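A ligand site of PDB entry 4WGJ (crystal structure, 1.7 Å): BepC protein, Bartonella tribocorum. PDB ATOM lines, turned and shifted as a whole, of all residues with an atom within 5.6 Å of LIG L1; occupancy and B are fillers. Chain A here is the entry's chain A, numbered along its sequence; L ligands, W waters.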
ATOM      1  N   PHE A  70     -16.841 -14.097  10.933  1.00  0.00           N
ATOM      2  CA  PHE A  70     -16.785 -14.748   9.615  1.00  0.00           C
ATOM      3  C   PHE A  70     -18.109 -15.288   9.054  1.00  0.00           C
ATOM      4  O   PHE A  70     -18.100 -15.880   7.970  1.00  0.00           O
ATOM      5  CB  PHE A  70     -15.754 -15.895   9.646  1.00  0.00           C
ATOM      6  CG  PHE A  70     -14.339 -15.416   9.718  1.00  0.00           C
ATOM      7  CD1 PHE A  70     -13.707 -14.949   8.578  1.00  0.00           C
ATOM      8  CD2 PHE A  70     -13.656 -15.387  10.919  1.00  0.00           C
ATOM      9  CE1 PHE A  70     -12.393 -14.476   8.629  1.00  0.00           C
ATOM     10  CE2 PHE A  70     -12.343 -14.905  10.980  1.00  0.00           C
ATOM     11  CZ  PHE A  70     -11.724 -14.452   9.813  1.00  0.00           C
ATOM     12  N   PRO A 100       1.880 -25.210   7.735  1.00  0.00           N
ATOM     13  CA  PRO A 100       2.231 -24.088   6.852  1.00  0.00           C
ATOM     14  C   PRO A 100       3.175 -24.540   5.739  1.00  0.00           C
ATOM     15  O   PRO A 100       4.150 -25.251   6.009  1.00  0.00           O
ATOM     16  CB  PRO A 100       2.918 -23.099   7.792  1.00  0.00           C
ATOM     17  CG  PRO A 100       2.413 -23.442   9.154  1.00  0.00           C
ATOM     18  CD  PRO A 100       2.182 -24.920   9.150  1.00  0.00           C
ATOM     19  N   TYR A 103       7.220 -25.200   5.824  1.00  0.00           N
ATOM     20  CA  TYR A 103       7.661 -25.373   7.215  1.00  0.00           C
ATOM     21  C   TYR A 103       7.403 -26.783   7.723  1.00  0.00           C
ATOM     22  O   TYR A 103       6.506 -27.470   7.237  1.00  0.00           O
ATOM     23  CB  TYR A 103       6.966 -24.356   8.126  1.00  0.00           C
ATOM     24  CG  TYR A 103       7.497 -22.972   7.900  1.00  0.00           C
ATOM     25  CD1 TYR A 103       8.653 -22.538   8.534  1.00  0.00           C
ATOM     26  CD2 TYR A 103       6.873 -22.108   6.996  1.00  0.00           C
ATOM     27  CE1 TYR A 103       9.167 -21.267   8.303  1.00  0.00           C
ATOM     28  CE2 TYR A 103       7.378 -20.842   6.768  1.00  0.00           C
ATOM     29  CZ  TYR A 103       8.517 -20.431   7.418  1.00  0.00           C
ATOM     30  OH  TYR A 103       9.022 -19.165   7.189  1.00  0.00           O
ATOM     31  N   ALA A 105       6.909 -27.852  11.165  1.00  0.00           N
ATOM     32  CA  ALA A 105       6.026 -28.056  12.321  1.00  0.00           C
ATOM     33  C   ALA A 105       4.571 -27.792  11.970  1.00  0.00           C
ATOM     34  O   ALA A 105       4.226 -26.709  11.494  1.00  0.00           O
ATOM     35  CB  ALA A 105       6.461 -27.176  13.486  1.00  0.00           C
ATOM     36  N   PHE A 107       0.357 -27.428  12.787  1.00  0.00           N
ATOM     37  CA  PHE A 107      -0.545 -27.026  13.856  1.00  0.00           C
ATOM     38  C   PHE A 107      -1.052 -28.275  14.577  1.00  0.00           C
ATOM     39  O   PHE A 107      -0.699 -29.390  14.203  1.00  0.00           O
ATOM     40  CB  PHE A 107      -1.698 -26.190  13.296  1.00  0.00           C
ATOM     41  CG  PHE A 107      -1.260 -24.910  12.648  1.00  0.00           C
ATOM     42  CD1 PHE A 107      -0.847 -23.836  13.422  1.00  0.00           C
ATOM     43  CD2 PHE A 107      -1.275 -24.781  11.259  1.00  0.00           C
ATOM     44  CE1 PHE A 107      -0.463 -22.641  12.822  1.00  0.00           C
ATOM     45  CE2 PHE A 107      -0.870 -23.598  10.663  1.00  0.00           C
ATOM     46  CZ  PHE A 107      -0.470 -22.520  11.441  1.00  0.00           C
ATOM     47  N   PHE A 146      -1.725 -16.641  23.696  1.00  0.00           N
ATOM     48  CA  PHE A 146      -1.837 -16.439  22.254  1.00  0.00           C
ATOM     49  C   PHE A 146      -1.090 -17.523  21.495  1.00  0.00           C
ATOM     50  O   PHE A 146      -1.559 -18.018  20.467  1.00  0.00           O
ATOM     51  CB  PHE A 146      -1.290 -15.065  21.866  1.00  0.00           C
ATOM     52  CG  PHE A 146      -1.494 -14.707  20.432  1.00  0.00           C
ATOM     53  CD1 PHE A 146      -2.772 -14.493  19.931  1.00  0.00           C
ATOM     54  CD2 PHE A 146      -0.414 -14.566  19.591  1.00  0.00           C
ATOM     55  CE1 PHE A 146      -2.963 -14.146  18.598  1.00  0.00           C
ATOM     56  CE2 PHE A 146      -0.587 -14.231  18.253  1.00  0.00           C
ATOM     57  CZ  PHE A 146      -1.858 -14.003  17.760  1.00  0.00           C
ATOM     58  N   GLU A 150      -2.580 -20.055  18.781  1.00  0.00           N
ATOM     59  CA  GLU A 150      -1.988 -20.084  17.443  1.00  0.00           C
ATOM     60  C   GLU A 150      -1.598 -21.528  17.088  1.00  0.00           C
ATOM     61  O   GLU A 150      -1.780 -21.959  15.939  1.00  0.00           O
ATOM     62  CB  GLU A 150      -0.778 -19.148  17.360  1.00  0.00           C
ATOM     63  CG  GLU A 150      -1.146 -17.673  17.143  1.00  0.00           C
ATOM     64  CD  GLU A 150      -1.772 -17.422  15.778  1.00  0.00           C
ATOM     65  OE1 GLU A 150      -1.171 -17.824  14.751  1.00  0.00           O
ATOM     66  OE2 GLU A 150      -2.873 -16.830  15.725  1.00  0.00           O
ATOM     67  N   HIS A 153      -4.893 -23.580  16.312  1.00  0.00           N
ATOM     68  CA  HIS A 153      -5.296 -23.240  14.941  1.00  0.00           C
ATOM     69  C   HIS A 153      -6.605 -23.949  14.605  1.00  0.00           C
ATOM     70  O   HIS A 153      -6.655 -24.735  13.655  1.00  0.00           O
ATOM     71  CB  HIS A 153      -4.170 -23.662  13.969  1.00  0.00           C
ATOM     72  CG  HIS A 153      -4.276 -23.084  12.579  1.00  0.00           C
ATOM     73  ND1 HIS A 153      -3.804 -21.832  12.255  1.00  0.00           N
ATOM     74  CD2 HIS A 153      -4.748 -23.617  11.426  1.00  0.00           C
ATOM     75  CE1 HIS A 153      -3.976 -21.610  10.969  1.00  0.00           C
ATOM     76  NE2 HIS A 153      -4.558 -22.681  10.436  1.00  0.00           N
ATOM     77  N   PHE A 155      -9.513 -23.499  13.295  1.00  0.00           N
ATOM     78  CA  PHE A 155     -10.407 -23.316  12.139  1.00  0.00           C
ATOM     79  C   PHE A 155      -9.705 -23.527  10.798  1.00  0.00           C
ATOM     80  O   PHE A 155      -8.481 -23.437  10.709  1.00  0.00           O
ATOM     81  CB  PHE A 155     -11.053 -21.912  12.177  1.00  0.00           C
ATOM     82  CG  PHE A 155     -11.693 -21.608  13.509  1.00  0.00           C
ATOM     83  CD1 PHE A 155     -12.964 -22.081  13.791  1.00  0.00           C
ATOM     84  CD2 PHE A 155     -11.009 -20.880  14.480  1.00  0.00           C
ATOM     85  CE1 PHE A 155     -13.561 -21.839  15.026  1.00  0.00           C
ATOM     86  CE2 PHE A 155     -11.589 -20.642  15.721  1.00  0.00           C
ATOM     87  CZ  PHE A 155     -12.874 -21.120  15.986  1.00  0.00           C
ATOM     88  N   ARG A 156     -10.486 -23.775   9.753  1.00  0.00           N
ATOM     89  CA  ARG A 156      -9.899 -23.934   8.416  1.00  0.00           C
ATOM     90  C   ARG A 156      -9.220 -22.636   7.955  1.00  0.00           C
ATOM     91  O   ARG A 156      -8.217 -22.654   7.254  1.00  0.00           O
ATOM     92  CB  ARG A 156     -10.974 -24.388   7.421  1.00  0.00           C
ATOM     93  CG  ARG A 156     -10.496 -24.471   5.962  1.00  0.00           C
ATOM     94  CD  ARG A 156      -9.313 -25.443   5.810  1.00  0.00           C
ATOM     95  NE  ARG A 156      -8.849 -25.487   4.417  1.00  0.00           N
ATOM     96  CZ  ARG A 156      -8.078 -24.558   3.843  1.00  0.00           C
ATOM     97  NH1 ARG A 156      -7.680 -23.501   4.538  1.00  0.00           N
ATOM     98  NH2 ARG A 156      -7.713 -24.700   2.565  1.00  0.00           N
ATOM     99  N   LYS A 157      -9.779 -21.507   8.394  1.00  0.00           N
ATOM    100  CA  LYS A 157      -9.270 -20.189   8.007  1.00  0.00           C
ATOM    101  C   LYS A 157      -9.816 -19.188   9.018  1.00  0.00           C
ATOM    102  O   LYS A 157     -10.814 -19.473   9.686  1.00  0.00           O
ATOM    103  CB  LYS A 157      -9.714 -19.814   6.575  1.00  0.00           C
ATOM    104  CG  LYS A 157      -8.922 -18.662   5.921  1.00  0.00           C
ATOM    105  CD  LYS A 157      -7.451 -19.058   5.753  1.00  0.00           C
ATOM    106  CE  LYS A 157      -6.687 -18.069   4.887  1.00  0.00           C
ATOM    107  NZ  LYS A 157      -6.666 -16.704   5.470  1.00  0.00           N
ATOM    108  N   GLY A 158      -9.154 -18.050   9.159  1.00  0.00           N
ATOM    109  CA  GLY A 158      -9.613 -17.020  10.080  1.00  0.00           C
ATOM    110  C   GLY A 158      -9.080 -17.170  11.495  1.00  0.00           C
ATOM    111  O   GLY A 158      -9.565 -16.526  12.434  1.00  0.00           O
ATOM    112  N   ASN A 159      -8.071 -18.007  11.670  1.00  0.00           N
ATOM    113  CA  ASN A 159      -7.502 -18.247  12.990  1.00  0.00           C
ATOM    114  C   ASN A 159      -6.834 -17.024  13.590  1.00  0.00           C
ATOM    115  O   ASN A 159      -7.042 -16.719  14.756  1.00  0.00           O
ATOM    116  CB  ASN A 159      -6.481 -19.383  12.930  1.00  0.00           C
ATOM    117  CG  ASN A 159      -7.143 -20.701  12.632  1.00  0.00           C
ATOM    118  OD1 ASN A 159      -7.717 -21.312  13.523  1.00  0.00           O
ATOM    119  ND2 ASN A 159      -7.071 -21.138  11.393  1.00  0.00           N
ATOM    120  N   GLY A 160      -6.024 -16.334  12.793  1.00  0.00           N
ATOM    121  CA  GLY A 160      -5.322 -15.152  13.267  1.00  0.00           C
ATOM    122  C   GLY A 160      -6.289 -14.106  13.750  1.00  0.00           C
ATOM    123  O   GLY A 160      -6.169 -13.561  14.845  1.00  0.00           O
ATOM    124  N   ARG A 161      -7.286 -13.806  12.921  1.00  0.00           N
ATOM    125  CA  ARG A 161      -8.236 -12.766  13.293  1.00  0.00           C
ATOM    126  C   ARG A 161      -9.065 -13.170  14.506  1.00  0.00           C
ATOM    127  O   ARG A 161      -9.299 -12.359  15.408  1.00  0.00           O
ATOM    128  CB  ARG A 161      -9.105 -12.411  12.088  1.00  0.00           C
ATOM    129  CG  ARG A 161      -8.332 -11.522  11.094  1.00  0.00           C
ATOM    130  CD  ARG A 161      -8.955 -11.428   9.707  1.00  0.00           C
ATOM    131  NE  ARG A 161      -8.750 -12.659   8.938  1.00  0.00           N
ATOM    132  CZ  ARG A 161      -9.190 -12.848   7.703  1.00  0.00           C
ATOM    133  NH1 ARG A 161      -9.873 -11.872   7.101  1.00  0.00           N
ATOM    134  NH2 ARG A 161      -8.974 -14.006   7.078  1.00  0.00           N
ATOM    135  N   ALA A 162      -9.507 -14.420  14.579  1.00  0.00           N
ATOM    136  CA  ALA A 162     -10.266 -14.823  15.748  1.00  0.00           C
ATOM    137  C   ALA A 162      -9.407 -14.812  17.009  1.00  0.00           C
ATOM    138  O   ALA A 162      -9.843 -14.361  18.079  1.00  0.00           O
ATOM    139  CB  ALA A 162     -10.891 -16.194  15.542  1.00  0.00           C
ATOM    140  N   ARG A 164      -6.666 -13.049  17.622  1.00  0.00           N
ATOM    141  CA  ARG A 164      -6.338 -11.681  18.035  1.00  0.00           C
ATOM    142  C   ARG A 164      -7.526 -11.029  18.754  1.00  0.00           C
ATOM    143  O   ARG A 164      -7.350 -10.358  19.769  1.00  0.00           O
ATOM    144  CB  ARG A 164      -5.879 -10.860  16.834  1.00  0.00           C
ATOM    145  CG  ARG A 164      -4.550 -11.395  16.292  1.00  0.00           C
ATOM    146  CD  ARG A 164      -3.818 -10.439  15.373  1.00  0.00           C
ATOM    147  NE  ARG A 164      -4.543 -10.174  14.144  1.00  0.00           N
ATOM    148  CZ  ARG A 164      -4.470 -10.922  13.041  1.00  0.00           C
ATOM    149  NH1 ARG A 164      -3.714 -12.025  13.011  1.00  0.00           N
ATOM    150  NH2 ARG A 164      -5.174 -10.570  11.973  1.00  0.00           N
ATOM    151  N   MET A 188       3.826  -9.836  12.846  1.00  0.00           N
ATOM    152  CA  MET A 188       3.068 -10.910  13.490  1.00  0.00           C
ATOM    153  C   MET A 188       3.539 -12.276  13.005  1.00  0.00           C
ATOM    154  O   MET A 188       3.736 -13.185  13.811  1.00  0.00           O
ATOM    155  CB  MET A 188       1.580 -10.748  13.222  1.00  0.00           C
ATOM    156  CG  MET A 188       0.753 -11.953  13.741  1.00  0.00           C
ATOM    157  SD  MET A 188       0.845 -12.114  15.545  1.00  0.00           S
ATOM    158  CE  MET A 188      -0.055 -10.642  15.987  1.00  0.00           C
ATOM    159  N   THR A 189       3.710 -12.414  11.693  1.00  0.00           N
ATOM    160  CA  THR A 189       4.154 -13.685  11.112  1.00  0.00           C
ATOM    161  C   THR A 189       5.503 -14.094  11.695  1.00  0.00           C
ATOM    162  O   THR A 189       5.686 -15.244  12.107  1.00  0.00           O
ATOM    163  CB  THR A 189       4.242 -13.578   9.586  1.00  0.00           C
ATOM    164  OG1 THR A 189       2.922 -13.429   9.057  1.00  0.00           O
ATOM    165  CG2 THR A 189       4.859 -14.835   9.003  1.00  0.00           C
ATOM    166  N   CYS A 192       4.994 -15.403  15.205  1.00  0.00           N
ATOM    167  CA  CYS A 192       4.324 -16.705  15.181  1.00  0.00           C
ATOM    168  C   CYS A 192       5.253 -17.826  14.742  1.00  0.00           C
ATOM    169  O   CYS A 192       5.289 -18.907  15.357  1.00  0.00           O
ATOM    170  CB  CYS A 192       3.103 -16.640  14.264  1.00  0.00           C
ATOM    171  SG  CYS A 192       1.733 -15.685  14.988  1.00  0.00           S
ATOM    172  N   ILE A 193       6.000 -17.573  13.670  1.00  0.00           N
ATOM    173  CA  ILE A 193       6.925 -18.576  13.138  1.00  0.00           C
ATOM    174  C   ILE A 193       8.051 -18.880  14.137  1.00  0.00           C
ATOM    175  O   ILE A 193       8.373 -20.041  14.390  1.00  0.00           O
ATOM    176  CB  ILE A 193       7.513 -18.121  11.792  1.00  0.00           C
ATOM    177  CG1 ILE A 193       6.411 -18.136  10.711  1.00  0.00           C
ATOM    178  CG2 ILE A 193       8.702 -18.998  11.376  1.00  0.00           C
ATOM    179  CD1 ILE A 193       6.891 -17.633   9.347  1.00  0.00           C
ATOM    180  N   MET A 196       6.455 -21.040  16.968  1.00  0.00           N
ATOM    181  CA  MET A 196       5.924 -22.369  16.681  1.00  0.00           C
ATOM    182  C   MET A 196       6.892 -23.248  15.905  1.00  0.00           C
ATOM    183  O   MET A 196       6.969 -24.457  16.130  1.00  0.00           O
ATOM    184  CB  MET A 196       4.607 -22.259  15.930  1.00  0.00           C
ATOM    185  CG  MET A 196       3.927 -23.599  15.764  1.00  0.00           C
ATOM    186  SD  MET A 196       2.318 -23.439  14.989  1.00  0.00           S
ATOM    187  CE  MET A 196       2.528 -24.614  13.653  1.00  0.00           C
ATOM    188  N   GLN A 197       7.628 -22.644  14.974  1.00  0.00           N
ATOM    189  CA  GLN A 197       8.550 -23.413  14.149  1.00  0.00           C
ATOM    190  C   GLN A 197       9.911 -23.599  14.813  1.00  0.00           C
ATOM    191  O   GLN A 197      10.572 -24.632  14.615  1.00  0.00           O
ATOM    192  CB  GLN A 197       8.755 -22.760  12.777  1.00  0.00           C
ATOM    193  CG  GLN A 197       7.491 -22.663  11.936  1.00  0.00           C
ATOM    194  CD  GLN A 197       6.891 -24.013  11.618  1.00  0.00           C
ATOM    195  OE1 GLN A 197       7.606 -24.994  11.424  1.00  0.00           O
ATOM    196  NE2 GLN A 197       5.555 -24.063  11.586  1.00  0.00           N
HETATM  197  P1  LIG L   1      -4.437 -13.267   9.170  1.00  0.00           P
HETATM  198  O1  LIG L   1      -5.348 -11.992   9.310  1.00  0.00           O
HETATM  199  O2  LIG L   1      -3.295 -12.906   8.258  1.00  0.00           O
HETATM  200  O3  LIG L   1      -3.887 -13.640  10.600  1.00  0.00           O
HETATM  201  P2  LIG L   1      -6.399 -15.512   9.150  1.00  0.00           P
HETATM  202  O4  LIG L   1      -7.143 -14.674  10.139  1.00  0.00           O
HETATM  203  O5  LIG L   1      -7.339 -16.105   8.050  1.00  0.00           O
HETATM  204  N1  LIG L   1      -5.211 -14.587   8.393  1.00  0.00           N
HETATM  205  P3  LIG L   1      -5.184 -18.042   9.216  1.00  0.00           P
HETATM  206  O6  LIG L   1      -4.672 -17.797   7.841  1.00  0.00           O
HETATM  207  O7  LIG L   1      -6.118 -19.233   9.380  1.00  0.00           O
HETATM  208  O8  LIG L   1      -5.802 -16.748   9.904  1.00  0.00           O
HETATM  209  O9  LIG L   1      -3.924 -18.231  10.173  1.00  0.00           O
HETATM  210  C1  LIG L   1      -2.890 -17.217  10.145  1.00  0.00           C
HETATM  211  C2  LIG L   1      -2.013 -17.316  11.368  1.00  0.00           C
HETATM  212  O10 LIG L   1      -1.001 -18.338  11.154  1.00  0.00           O
HETATM  213  C3  LIG L   1      -1.263 -16.025  11.702  1.00  0.00           C
HETATM  214  O11 LIG L   1      -1.260 -15.748  13.106  1.00  0.00           O
HETATM  215  C4  LIG L   1       0.144 -16.301  11.177  1.00  0.00           C
HETATM  216  O12 LIG L   1       1.153 -15.535  11.827  1.00  0.00           O
HETATM  217  C5  LIG L   1       0.270 -17.796  11.470  1.00  0.00           C
HETATM  218  N2  LIG L   1       1.310 -18.460  10.683  1.00  0.00           N
HETATM  219  C6  LIG L   1       1.637 -18.213   9.376  1.00  0.00           C
HETATM  220  N3  LIG L   1       2.628 -18.940   8.928  1.00  0.00           N
HETATM  221  C7  LIG L   1       2.990 -19.716  10.018  1.00  0.00           C
HETATM  222  C8  LIG L   1       3.980 -20.694  10.209  1.00  0.00           C
HETATM  223  N4  LIG L   1       4.828 -21.087   9.252  1.00  0.00           N
HETATM  224  N5  LIG L   1       4.070 -21.273  11.427  1.00  0.00           N
HETATM  225  C9  LIG L   1       3.230 -20.888  12.393  1.00  0.00           C
HETATM  226  N6  LIG L   1       2.261 -19.979  12.331  1.00  0.00           N
HETATM  227  C10 LIG L   1       2.186 -19.426  11.109  1.00  0.00           C
HETATM  228  N1  LG2 L   2      -1.722  -9.645  10.171  1.00  0.00           N
HETATM  229  C1  LG2 L   2      -1.982  -8.285  10.622  1.00  0.00           C
HETATM  230  C2  LG2 L   2      -1.912  -8.163  12.130  1.00  0.00           C
HETATM  231  O1  LG2 L   2      -2.130  -7.089  12.703  1.00  0.00           O
HETATM  232  O2  LG2 L   2      -1.651  -9.143  12.811  1.00  0.00           O
HETATM  233  O   HOH W   1      -2.304 -13.903  14.390  1.00  0.00           O
HETATM  234  O   HOH W   2       4.267 -19.436   6.623  1.00  0.00           O
HETATM  235  O   HOH W   3      -0.558 -16.280   7.646  1.00  0.00           O
HETATM  236  O   HOH W   4      -2.829 -16.004   6.565  1.00  0.00           O
HETATM  237  O   HOH W   5      -2.641 -18.610   6.606  1.00  0.00           O
HETATM  238  O   HOH W   6       0.890 -19.284  14.606  1.00  0.00           O
HETATM  239  O   HOH W   7      -5.659 -21.706   7.985  1.00  0.00           O
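OE1 of Glu 150 is in hydrogen-bond range of O11 of LIG L1 (2.7 Å).
NZ of Lys 157 lies within salt-bridge range of O5 of LIG L1.
The backbone NH (N) of Arg 161 is in hydrogen-bond range of an oxygen (O4) of LIG L1 (2.9 Å).
The guanidinium group (NH2) of Arg 161 is in salt-bridge range of an oxygen (O5) of LIG L1 (2.8 Å).
O5 of LIG L1 sits at hydrogen-bond distance from N of Gly 158, 2.9 Å away.
NH1 of Arg 164 lies within salt-bridge range of O3 of LIG L1, at 2.9 Å.
N of Gly 160 lies within hydrogen-bond range of O8 of LIG L1, at 2.9 Å.
The backbone NH (N) of Asn 159 lies within hydrogen-bond range of an oxygen (O8) of LIG L1 (3.1 Å).
The side-chain amide nitrogen (ND2) of Asn 159 sits at hydrogen-bond distance from an oxygen (O7) of LIG L1 (2.9 Å).
N5 of LIG L1 lies within hydrogen-bond range of NE2 of Gln 197 (3.2 Å).
An oxygen (O12) of LIG L1 is in hydrogen-bond range of the side-chain sulfur (SG) of Cys 192.
O2 of LG2 L2 is in salt-bridge range of NE of Arg 164 (3.3 Å).
The side-chain carboxylate (OE1) of Glu 150 is in hydrogen-bond range of the side-chain sulfur (SG) of Cys 192 (3.6 Å).
The guanidinium group of Arg 164 sits close to the backbone carbonyl oxygen of Gly 160.
A ring nitrogen (NE2) of His 153 is in hydrogen-bond range of the side-chain amide nitrogen of Asn 159, at 3.1 Å.
ND2 of Asn 159 sits at hydrogen-bond distance from O of Phe 155 (2.8 Å).
The side-chain amide oxygen of Gln 197 is in hydrogen-bond range of the backbone NH of Ala 105 (3.0 Å).
The side-chain sulfur (SG) of Cys 192 sits at hydrogen-bond distance from the backbone carbonyl oxygen (O) of Met 188, at 3.4 Å.
Merely in contact with LIG L1: Pro 100 (3.1 Å), Tyr 103 (3.2 Å), His 153 (3.5 Å), Ile 193 (3.6 Å), Thr 189 (3.6 Å), Met 196 (3.8 Å) and Phe 107 (3.8 Å).
Hydrophobic or aromatic side chains within 4 Å of LIG L1: Pro 100, Tyr 103, Phe 107, His 153, Ile 193 and Met 196.
Of the 23 residues printed, 16 come within 4 Å of LIG L1.
Water W1 lies within hydrogen-bond range of an oxygen (O11) of LIG L1, the guanidinium group of Arg 164 and the side-chain carboxylate of Glu 150.
Water W6 lies within hydrogen-bond range of the side-chain carboxylate of Glu 150, a nitrogen (N6) of LIG L1 and the side-chain sulfur of Cys 192.
Water W7 lies within hydrogen-bond range of O of Arg 156 (2.8 Å), NE2 of His 153 (2.9 Å) and O7 of LIG L1 (2.9 Å).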
